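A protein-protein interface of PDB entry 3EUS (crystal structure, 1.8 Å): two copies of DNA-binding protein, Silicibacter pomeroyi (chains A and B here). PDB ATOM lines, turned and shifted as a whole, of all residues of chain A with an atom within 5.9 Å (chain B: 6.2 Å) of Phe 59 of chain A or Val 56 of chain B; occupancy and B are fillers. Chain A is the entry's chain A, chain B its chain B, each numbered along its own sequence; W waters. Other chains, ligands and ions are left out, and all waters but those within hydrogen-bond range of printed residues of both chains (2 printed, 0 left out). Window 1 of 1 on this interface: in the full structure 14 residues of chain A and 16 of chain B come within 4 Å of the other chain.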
ATOM      1  N   LEU A  15      16.631  27.128 -12.224  1.00  0.00           N
ATOM      2  CA  LEU A  15      16.979  26.465 -10.993  1.00  0.00           C
ATOM      3  C   LEU A  15      18.505  26.377 -10.931  1.00  0.00           C
ATOM      4  O   LEU A  15      19.135  26.696  -9.913  1.00  0.00           O
ATOM      5  CB  LEU A  15      16.375  25.074 -10.951  1.00  0.00           C
ATOM      6  CG  LEU A  15      16.855  24.175  -9.824  1.00  0.00           C
ATOM      7  CD1 LEU A  15      16.644  24.813  -8.404  1.00  0.00           C
ATOM      8  CD2 LEU A  15      16.145  22.800  -9.905  1.00  0.00           C
ATOM      9  N   LEU A  19      21.054  27.673  -8.163  1.00  0.00           N
ATOM     10  CA  LEU A  19      21.944  26.758  -7.404  1.00  0.00           C
ATOM     11  C   LEU A  19      23.358  27.294  -7.442  1.00  0.00           C
ATOM     12  O   LEU A  19      24.072  27.398  -6.412  1.00  0.00           O
ATOM     13  CB  LEU A  19      21.877  25.394  -7.991  1.00  0.00           C
ATOM     14  CG  LEU A  19      20.608  24.616  -7.674  1.00  0.00           C
ATOM     15  CD1 LEU A  19      20.644  23.314  -8.479  1.00  0.00           C
ATOM     16  CD2 LEU A  19      20.530  24.390  -6.182  1.00  0.00           C
ATOM     17  N   LEU A  54      18.504  16.966  -9.835  1.00  0.00           N
ATOM     18  CA  LEU A  54      18.523  17.160  -8.361  1.00  0.00           C
ATOM     19  C   LEU A  54      17.174  16.792  -7.769  1.00  0.00           C
ATOM     20  O   LEU A  54      16.157  17.297  -8.199  1.00  0.00           O
ATOM     21  CB  LEU A  54      18.875  18.626  -8.039  1.00  0.00           C
ATOM     22  CG  LEU A  54      19.649  18.932  -6.772  1.00  0.00           C
ATOM     23  CD1 LEU A  54      21.067  18.387  -6.832  1.00  0.00           C
ATOM     24  CD2 LEU A  54      19.664  20.420  -6.458  1.00  0.00           C
ATOM     25  N   ASP A  55      17.113  15.915  -6.765  1.00  0.00           N
ATOM     26  CA  ASP A  55      15.855  15.718  -6.082  1.00  0.00           C
ATOM     27  C   ASP A  55      15.664  16.775  -4.961  1.00  0.00           C
ATOM     28  O   ASP A  55      16.541  17.626  -4.755  1.00  0.00           O
ATOM     29  CB  ASP A  55      15.629  14.253  -5.606  1.00  0.00           C
ATOM     30  CG  ASP A  55      16.423  13.863  -4.364  1.00  0.00           C
ATOM     31  OD1 ASP A  55      16.858  14.728  -3.567  1.00  0.00           O
ATOM     32  OD2 ASP A  55      16.607  12.622  -4.151  1.00  0.00           O
ATOM     33  N   VAL A  56      14.507  16.769  -4.301  1.00  0.00           N
ATOM     34  CA  VAL A  56      14.185  17.778  -3.286  1.00  0.00           C
ATOM     35  C   VAL A  56      15.126  17.700  -2.080  1.00  0.00           C
ATOM     36  O   VAL A  56      15.489  18.725  -1.505  1.00  0.00           O
ATOM     37  CB  VAL A  56      12.701  17.690  -2.810  1.00  0.00           C
ATOM     38  CG1 VAL A  56      12.433  18.685  -1.596  1.00  0.00           C
ATOM     39  CG2 VAL A  56      11.825  18.017  -3.987  1.00  0.00           C
ATOM     40  N   ILE A  57      15.503  16.480  -1.676  1.00  0.00           N
ATOM     41  CA  ILE A  57      16.291  16.291  -0.486  1.00  0.00           C
ATOM     42  C   ILE A  57      17.709  16.832  -0.791  1.00  0.00           C
ATOM     43  O   ILE A  57      18.305  17.553   0.053  1.00  0.00           O
ATOM     44  CB  ILE A  57      16.348  14.802  -0.051  1.00  0.00           C
ATOM     45  CG1 ILE A  57      15.027  14.286   0.556  1.00  0.00           C
ATOM     46  CG2 ILE A  57      17.438  14.614   0.959  1.00  0.00           C
ATOM     47  CD1 ILE A  57      13.848  15.082   0.338  1.00  0.00           C
ATOM     48  N   GLU A  58      18.217  16.532  -1.994  1.00  0.00           N
ATOM     49  CA  GLU A  58      19.544  17.021  -2.436  1.00  0.00           C
ATOM     50  C   GLU A  58      19.474  18.573  -2.504  1.00  0.00           C
ATOM     51  O   GLU A  58      20.413  19.249  -2.108  1.00  0.00           O
ATOM     52  CB  GLU A  58      19.927  16.414  -3.780  1.00  0.00           C
ATOM     53  CG  GLU A  58      20.165  14.910  -3.719  1.00  0.00           C
ATOM     54  CD  GLU A  58      20.255  14.218  -5.082  1.00  0.00           C
ATOM     55  OE1 GLU A  58      19.736  14.735  -6.056  1.00  0.00           O
ATOM     56  OE2 GLU A  58      20.915  13.156  -5.190  1.00  0.00           O
ATOM     57  N   PHE A  59      18.367  19.134  -3.003  1.00  0.00           N
ATOM     58  CA  PHE A  59      18.197  20.580  -3.049  1.00  0.00           C
ATOM     59  C   PHE A  59      18.260  21.183  -1.660  1.00  0.00           C
ATOM     60  O   PHE A  59      18.901  22.222  -1.443  1.00  0.00           O
ATOM     61  CB  PHE A  59      16.871  20.886  -3.773  1.00  0.00           C
ATOM     62  CG  PHE A  59      16.434  22.288  -3.712  1.00  0.00           C
ATOM     63  CD1 PHE A  59      17.087  23.264  -4.458  1.00  0.00           C
ATOM     64  CD2 PHE A  59      15.259  22.659  -3.030  1.00  0.00           C
ATOM     65  CE1 PHE A  59      16.652  24.543  -4.467  1.00  0.00           C
ATOM     66  CE2 PHE A  59      14.830  24.031  -3.010  1.00  0.00           C
ATOM     67  CZ  PHE A  59      15.543  24.965  -3.734  1.00  0.00           C
ATOM     68  N   ALA A  60      17.498  20.625  -0.725  1.00  0.00           N
ATOM     69  CA  ALA A  60      17.523  21.097   0.652  1.00  0.00           C
ATOM     70  C   ALA A  60      18.952  21.119   1.175  1.00  0.00           C
ATOM     71  O   ALA A  60      19.377  22.107   1.800  1.00  0.00           O
ATOM     72  CB  ALA A  60      16.549  20.195   1.556  1.00  0.00           C
ATOM     73  N   LYS A  61      19.705  20.031   0.974  1.00  0.00           N
ATOM     74  CA  LYS A  61      21.034  19.974   1.525  1.00  0.00           C
ATOM     75  C   LYS A  61      21.977  21.010   0.866  1.00  0.00           C
ATOM     76  O   LYS A  61      22.827  21.610   1.517  1.00  0.00           O
ATOM     77  CB  LYS A  61      21.591  18.563   1.382  1.00  0.00           C
ATOM     78  CG  LYS A  61      20.883  17.489   2.322  1.00  0.00           C
ATOM     79  CD  LYS A  61      21.350  16.098   1.943  1.00  0.00           C
ATOM     80  CE  LYS A  61      20.753  14.987   2.857  1.00  0.00           C
ATOM     81  NZ  LYS A  61      21.288  13.599   2.587  1.00  0.00           N
ATOM     82  N   TRP A  62      21.854  21.147  -0.424  1.00  0.00           N
ATOM     83  CA  TRP A  62      22.683  22.124  -1.227  1.00  0.00           C
ATOM     84  C   TRP A  62      22.403  23.532  -0.692  1.00  0.00           C
ATOM     85  O   TRP A  62      23.309  24.307  -0.412  1.00  0.00           O
ATOM     86  CB  TRP A  62      22.247  22.055  -2.688  1.00  0.00           C
ATOM     87  CG  TRP A  62      23.006  22.904  -3.691  1.00  0.00           C
ATOM     88  CD1 TRP A  62      22.987  24.264  -3.804  1.00  0.00           C
ATOM     89  CD2 TRP A  62      23.737  22.424  -4.814  1.00  0.00           C
ATOM     90  NE1 TRP A  62      23.717  24.666  -4.904  1.00  0.00           N
ATOM     91  CE2 TRP A  62      24.197  23.558  -5.539  1.00  0.00           C
ATOM     92  CE3 TRP A  62      24.085  21.159  -5.268  1.00  0.00           C
ATOM     93  CZ2 TRP A  62      24.987  23.444  -6.674  1.00  0.00           C
ATOM     94  CZ3 TRP A  62      24.830  21.051  -6.409  1.00  0.00           C
ATOM     95  CH2 TRP A  62      25.283  22.203  -7.105  1.00  0.00           C
ATOM     96  N   MET A  63      21.123  23.888  -0.567  1.00  0.00           N
ATOM     97  CA  MET A  63      20.780  25.232  -0.151  1.00  0.00           C
ATOM     98  C   MET A  63      21.223  25.504   1.280  1.00  0.00           C
ATOM     99  O   MET A  63      21.708  26.563   1.569  1.00  0.00           O
ATOM    100  CB  MET A  63      19.274  25.510  -0.370  1.00  0.00           C
ATOM    101  CG  MET A  63      18.910  25.549  -1.879  1.00  0.00           C
ATOM    102  SD  MET A  63      19.811  26.684  -2.976  1.00  0.00           S
ATOM    103  CE  MET A  63      19.438  28.283  -2.239  1.00  0.00           C
ATOM    104  N   ALA A  64      21.082  24.526   2.167  1.00  0.00           N
ATOM    105  CA  ALA A  64      21.593  24.651   3.519  1.00  0.00           C
ATOM    106  C   ALA A  64      23.094  24.795   3.581  1.00  0.00           C
ATOM    107  O   ALA A  64      23.602  25.576   4.408  1.00  0.00           O
ATOM    108  CB  ALA A  64      21.174  23.391   4.403  1.00  0.00           C
ATOM    109  N   VAL A  72      14.901  29.892  -0.457  1.00  0.00           N
ATOM    110  CA  VAL A  72      14.220  28.688  -0.952  1.00  0.00           C
ATOM    111  C   VAL A  72      12.785  29.049  -1.441  1.00  0.00           C
ATOM    112  O   VAL A  72      12.377  28.665  -2.533  1.00  0.00           O
ATOM    113  CB  VAL A  72      14.238  27.546   0.110  1.00  0.00           C
ATOM    114  CG1 VAL A  72      13.220  26.436  -0.220  1.00  0.00           C
ATOM    115  CG2 VAL A  72      15.710  26.838   0.176  1.00  0.00           C
ATOM    116  N   ILE A  75      12.839  30.913  -4.812  1.00  0.00           N
ATOM    117  CA  ILE A  75      13.261  29.987  -5.908  1.00  0.00           C
ATOM    118  C   ILE A  75      12.067  29.098  -6.354  1.00  0.00           C
ATOM    119  O   ILE A  75      11.693  29.070  -7.530  1.00  0.00           O
ATOM    120  CB  ILE A  75      14.451  29.154  -5.475  1.00  0.00           C
ATOM    121  CG1 ILE A  75      15.689  30.076  -5.248  1.00  0.00           C
ATOM    122  CG2 ILE A  75      14.733  28.018  -6.533  1.00  0.00           C
ATOM    123  CD1 ILE A  75      16.861  29.399  -4.581  1.00  0.00           C
ATOM    124  N   VAL A  76      11.415  28.469  -5.381  1.00  0.00           N
ATOM    125  CA  VAL A  76      10.363  27.497  -5.651  1.00  0.00           C
ATOM    126  C   VAL A  76       9.112  28.198  -6.191  1.00  0.00           C
ATOM    127  O   VAL A  76       8.533  27.760  -7.174  1.00  0.00           O
ATOM    128  CB  VAL A  76      10.057  26.664  -4.364  1.00  0.00           C
ATOM    129  CG1 VAL A  76       8.736  25.825  -4.540  1.00  0.00           C
ATOM    130  CG2 VAL A  76      11.242  25.842  -3.881  1.00  0.00           C
ATOM    131  N   ILE A  79       9.875  29.240  -9.832  1.00  0.00           N
ATOM    132  CA  ILE A  79       9.748  28.053 -10.686  1.00  0.00           C
ATOM    133  C   ILE A  79       8.282  27.752 -10.934  1.00  0.00           C
ATOM    134  O   ILE A  79       7.900  27.561 -12.117  1.00  0.00           O
ATOM    135  CB  ILE A  79      10.483  26.819 -10.132  1.00  0.00           C
ATOM    136  CG1 ILE A  79      12.013  27.024 -10.190  1.00  0.00           C
ATOM    137  CG2 ILE A  79      10.038  25.555 -10.901  1.00  0.00           C
ATOM    138  CD1 ILE A  79      12.725  26.181  -9.271  1.00  0.00           C
ATOM    139  N   LEU B  54      10.251  13.147  -6.482  1.00  0.00           N
ATOM    140  CA  LEU B  54      10.057  14.388  -7.222  1.00  0.00           C
ATOM    141  C   LEU B  54      11.369  15.084  -7.445  1.00  0.00           C
ATOM    142  O   LEU B  54      12.215  15.103  -6.544  1.00  0.00           O
ATOM    143  CB  LEU B  54       9.191  15.368  -6.420  1.00  0.00           C
ATOM    144  CG  LEU B  54       7.722  15.057  -6.219  1.00  0.00           C
ATOM    145  CD1 LEU B  54       7.014  16.222  -5.508  1.00  0.00           C
ATOM    146  CD2 LEU B  54       7.080  14.705  -7.475  1.00  0.00           C
ATOM    147  N   ASP B  55      11.521  15.748  -8.583  1.00  0.00           N
ATOM    148  CA  ASP B  55      12.531  16.798  -8.643  1.00  0.00           C
ATOM    149  C   ASP B  55      12.023  18.087  -8.104  1.00  0.00           C
ATOM    150  O   ASP B  55      10.842  18.218  -7.698  1.00  0.00           O
ATOM    151  CB  ASP B  55      13.166  16.889 -10.063  1.00  0.00           C
ATOM    152  CG  ASP B  55      12.255  17.498 -11.099  1.00  0.00           C
ATOM    153  OD1 ASP B  55      11.326  18.263 -10.797  1.00  0.00           O
ATOM    154  OD2 ASP B  55      12.515  17.246 -12.301  1.00  0.00           O
ATOM    155  N   VAL B  56      12.878  19.113  -8.104  1.00  0.00           N
ATOM    156  CA  VAL B  56      12.482  20.412  -7.580  1.00  0.00           C
ATOM    157  C   VAL B  56      11.389  21.134  -8.314  1.00  0.00           C
ATOM    158  O   VAL B  56      10.543  21.853  -7.701  1.00  0.00           O
ATOM    159  CB  VAL B  56      13.683  21.371  -7.481  1.00  0.00           C
ATOM    160  CG1 VAL B  56      13.203  22.745  -7.091  1.00  0.00           C
ATOM    161  CG2 VAL B  56      14.740  20.760  -6.532  1.00  0.00           C
ATOM    162  N   ILE B  57      11.380  20.965  -9.631  1.00  0.00           N
ATOM    163  CA  ILE B  57      10.397  21.600 -10.448  1.00  0.00           C
ATOM    164  C   ILE B  57       9.037  20.957 -10.170  1.00  0.00           C
ATOM    165  O   ILE B  57       8.054  21.671  -9.958  1.00  0.00           O
ATOM    166  CB  ILE B  57      10.773  21.515 -11.949  1.00  0.00           C
ATOM    167  CG1 ILE B  57      11.899  22.499 -12.298  1.00  0.00           C
ATOM    168  CG2 ILE B  57       9.649  21.943 -12.774  1.00  0.00           C
ATOM    169  CD1 ILE B  57      12.959  22.499 -11.381  1.00  0.00           C
ATOM    170  N   GLU B  58       9.013  19.625 -10.107  1.00  0.00           N
ATOM    171  CA  GLU B  58       7.760  18.919  -9.793  1.00  0.00           C
ATOM    172  C   GLU B  58       7.225  19.291  -8.365  1.00  0.00           C
ATOM    173  O   GLU B  58       6.029  19.537  -8.148  1.00  0.00           O
ATOM    174  CB  GLU B  58       7.984  17.417  -9.940  1.00  0.00           C
ATOM    175  CG  GLU B  58       8.209  16.993 -11.359  1.00  0.00           C
ATOM    176  CD  GLU B  58       8.736  15.602 -11.473  1.00  0.00           C
ATOM    177  OE1 GLU B  58       9.374  15.108 -10.552  1.00  0.00           O
ATOM    178  OE2 GLU B  58       8.558  14.992 -12.531  1.00  0.00           O
ATOM    179  N   PHE B  59       8.166  19.369  -7.415  1.00  0.00           N
ATOM    180  CA  PHE B  59       7.905  19.835  -6.073  1.00  0.00           C
ATOM    181  C   PHE B  59       7.239  21.232  -6.067  1.00  0.00           C
ATOM    182  O   PHE B  59       6.199  21.430  -5.438  1.00  0.00           O
ATOM    183  CB  PHE B  59       9.189  19.813  -5.247  1.00  0.00           C
ATOM    184  CG  PHE B  59       9.031  20.362  -3.858  1.00  0.00           C
ATOM    185  CD1 PHE B  59       8.281  19.700  -2.923  1.00  0.00           C
ATOM    186  CD2 PHE B  59       9.585  21.597  -3.512  1.00  0.00           C
ATOM    187  CE1 PHE B  59       8.133  20.252  -1.596  1.00  0.00           C
ATOM    188  CE2 PHE B  59       9.488  22.094  -2.174  1.00  0.00           C
ATOM    189  CZ  PHE B  59       8.778  21.445  -1.243  1.00  0.00           C
ATOM    190  N   ALA B  60       7.830  22.186  -6.767  1.00  0.00           N
ATOM    191  CA  ALA B  60       7.266  23.524  -6.927  1.00  0.00           C
ATOM    192  C   ALA B  60       5.830  23.536  -7.476  1.00  0.00           C
ATOM    193  O   ALA B  60       4.925  24.222  -6.956  1.00  0.00           O
ATOM    194  CB  ALA B  60       8.179  24.359  -7.829  1.00  0.00           C
ATOM    195  N   LYS B  61       5.625  22.781  -8.558  1.00  0.00           N
ATOM    196  CA  LYS B  61       4.348  22.692  -9.164  1.00  0.00           C
ATOM    197  C   LYS B  61       3.327  22.058  -8.230  1.00  0.00           C
ATOM    198  O   LYS B  61       2.202  22.576  -8.106  1.00  0.00           O
ATOM    199  CB  LYS B  61       4.406  21.982 -10.496  1.00  0.00           C
ATOM    200  CG  LYS B  61       5.216  22.749 -11.559  1.00  0.00           C
ATOM    201  CD  LYS B  61       5.413  21.902 -12.807  1.00  0.00           C
ATOM    202  CE  LYS B  61       6.197  22.618 -13.949  1.00  0.00           C
ATOM    203  NZ  LYS B  61       6.387  21.696 -15.146  1.00  0.00           N
ATOM    204  N   VAL B  76      11.449  22.440   3.501  1.00  0.00           N
ATOM    205  CA  VAL B  76      12.816  22.274   2.995  1.00  0.00           C
ATOM    206  C   VAL B  76      13.855  22.452   4.113  1.00  0.00           C
ATOM    207  O   VAL B  76      14.882  21.693   4.202  1.00  0.00           O
ATOM    208  CB  VAL B  76      13.046  23.239   1.803  1.00  0.00           C
ATOM    209  CG1 VAL B  76      14.540  23.320   1.449  1.00  0.00           C
ATOM    210  CG2 VAL B  76      12.285  22.784   0.572  1.00  0.00           C
HETATM  211  O   HOH W   1      15.509  19.454  -9.746  1.00  0.00           O
HETATM  212  O   HOH W   2      12.661  14.389  -3.965  1.00  0.00           O
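The side-chain carboxylate of Asp 55 of chain A is in hydrogen-bond range of the backbone NH of Ile 57 of chain A (2.9 Å).
The side-chain carboxylate (OD1) of Asp 55 of chain A lies within hydrogen-bond range of the backbone NH (N) of Glu 58 of chain A (2.8 Å).
N of Ile 57 of chain B sits at hydrogen-bond distance from OD1 of Asp 55 of chain B (2.9 Å).
N of Glu 58 of chain B lies within hydrogen-bond range of OD1 of Asp 55 of chain B (2.8 Å).
Among the printed residues, merely in contact across the chains: Val 56 of chain A with Phe 59 of chain B (3.4 Å), Ala 60 of chain A with Val 76 of chain B (3.5 Å), Val 76 of chain A with Ala 60 of chain B (3.5 Å), Phe 59 of chain A with Val 56 of chain B (3.5 Å), Leu 15 of chain A with Ile 57 of chain B (3.5 Å), Leu 54 of chain A with Asp 55 of chain B (3.5 Å), Val 56 of chain A with Leu 54 of chain B (3.6 Å), Asp 55 of chain A with Leu 54 of chain B (3.6 Å), Leu 15 of chain A with Val 56 of chain B (3.7 Å), Leu 54 of chain A with Val 56 of chain B (3.7 Å), Val 72 of chain A with Val 76 of chain B (3.8 Å), Ile 79 of chain A with Ala 60 of chain B (3.8 Å), Ile 79 of chain A with Ile 57 of chain B (3.8 Å) and Val 56 of chain A with Asp 55 of chain B (3.8 Å).
Printed residues of chain B within 4 Å of Leu 15 of chain A: Val 56 and Ile 57.
Of the printed residues of chain B, Asp 55 of chain A touches Leu 54.
Printed residues of chain B within 4 Å of Phe 59 of chain A: Val 56.
Of the printed residues of chain A, Val 56 of chain B touches Leu 15, Leu 54 and Phe 59.
Of the printed residues of chain A, Ile 57 of chain B touches Leu 15 (3.5 Å) and Ile 79 (3.8 Å).
Printed residues of chain A within 4 Å of Ala 60 of chain B: Val 76 and Ile 79.
The nearest residue of chain B that does not touch Phe 59 of chain A is Val 76 of chain B (4.5 Å).
The nearest residue of chain A that does not touch Val 56 of chain B is Asp 55 of chain A (4.03 Å).
The nearest printed residue of chain B that does not touch Ile 79 of chain A is Val 56 of chain B (4.1 Å).
Of the 9 printed residues of chain B, 7 touch a printed residue of chain A.
Hydrophobic or aromatic side chains of chain B that line the printed part of chain A: Val 56, Ile 57, Phe 59, Ala 60 and Val 76.
Printed residues of chain A that touch a printed residue of chain B: Leu 15, Leu 54, Asp 55, Val 56, Phe 59, Ala 60, Val 72, Val 76 and Ile 79.
Among the printed residues, no Asp or Glu carboxylate lies within 4 Å of a Lys or Arg side-chain nitrogen of the other chain.
Leu 54 of chain A touches Val 56 of chain B, and with the chains exchanged Val 56 of chain A touches Leu 54 of chain B.
Val 56 of chain A touches Asp 55 of chain B, but with the chains exchanged Asp 55 of chain A does not touch Val 56 of chain B (4.03 Å).
Val 56 of chain A touches Phe 59 of chain B, and with the chains exchanged Phe 59 of chain A touches Val 56 of chain B.
Ala 60 of chain A touches Val 76 of chain B, and with the chains exchanged Val 76 of chain A touches Ala 60 of chain B.
9 positions are printed for both chains.
Water W2 bridges the backbone carbonyl oxygen (O) of Leu 54 of chain B (2.7 Å) and the backbone NH (N) of Val 56 of chain A (3.0 Å).
Water W1 lies within hydrogen-bond range of the backbone carbonyl oxygen of Leu 54 of chain A and the backbone NH of Val 56 of chain B.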
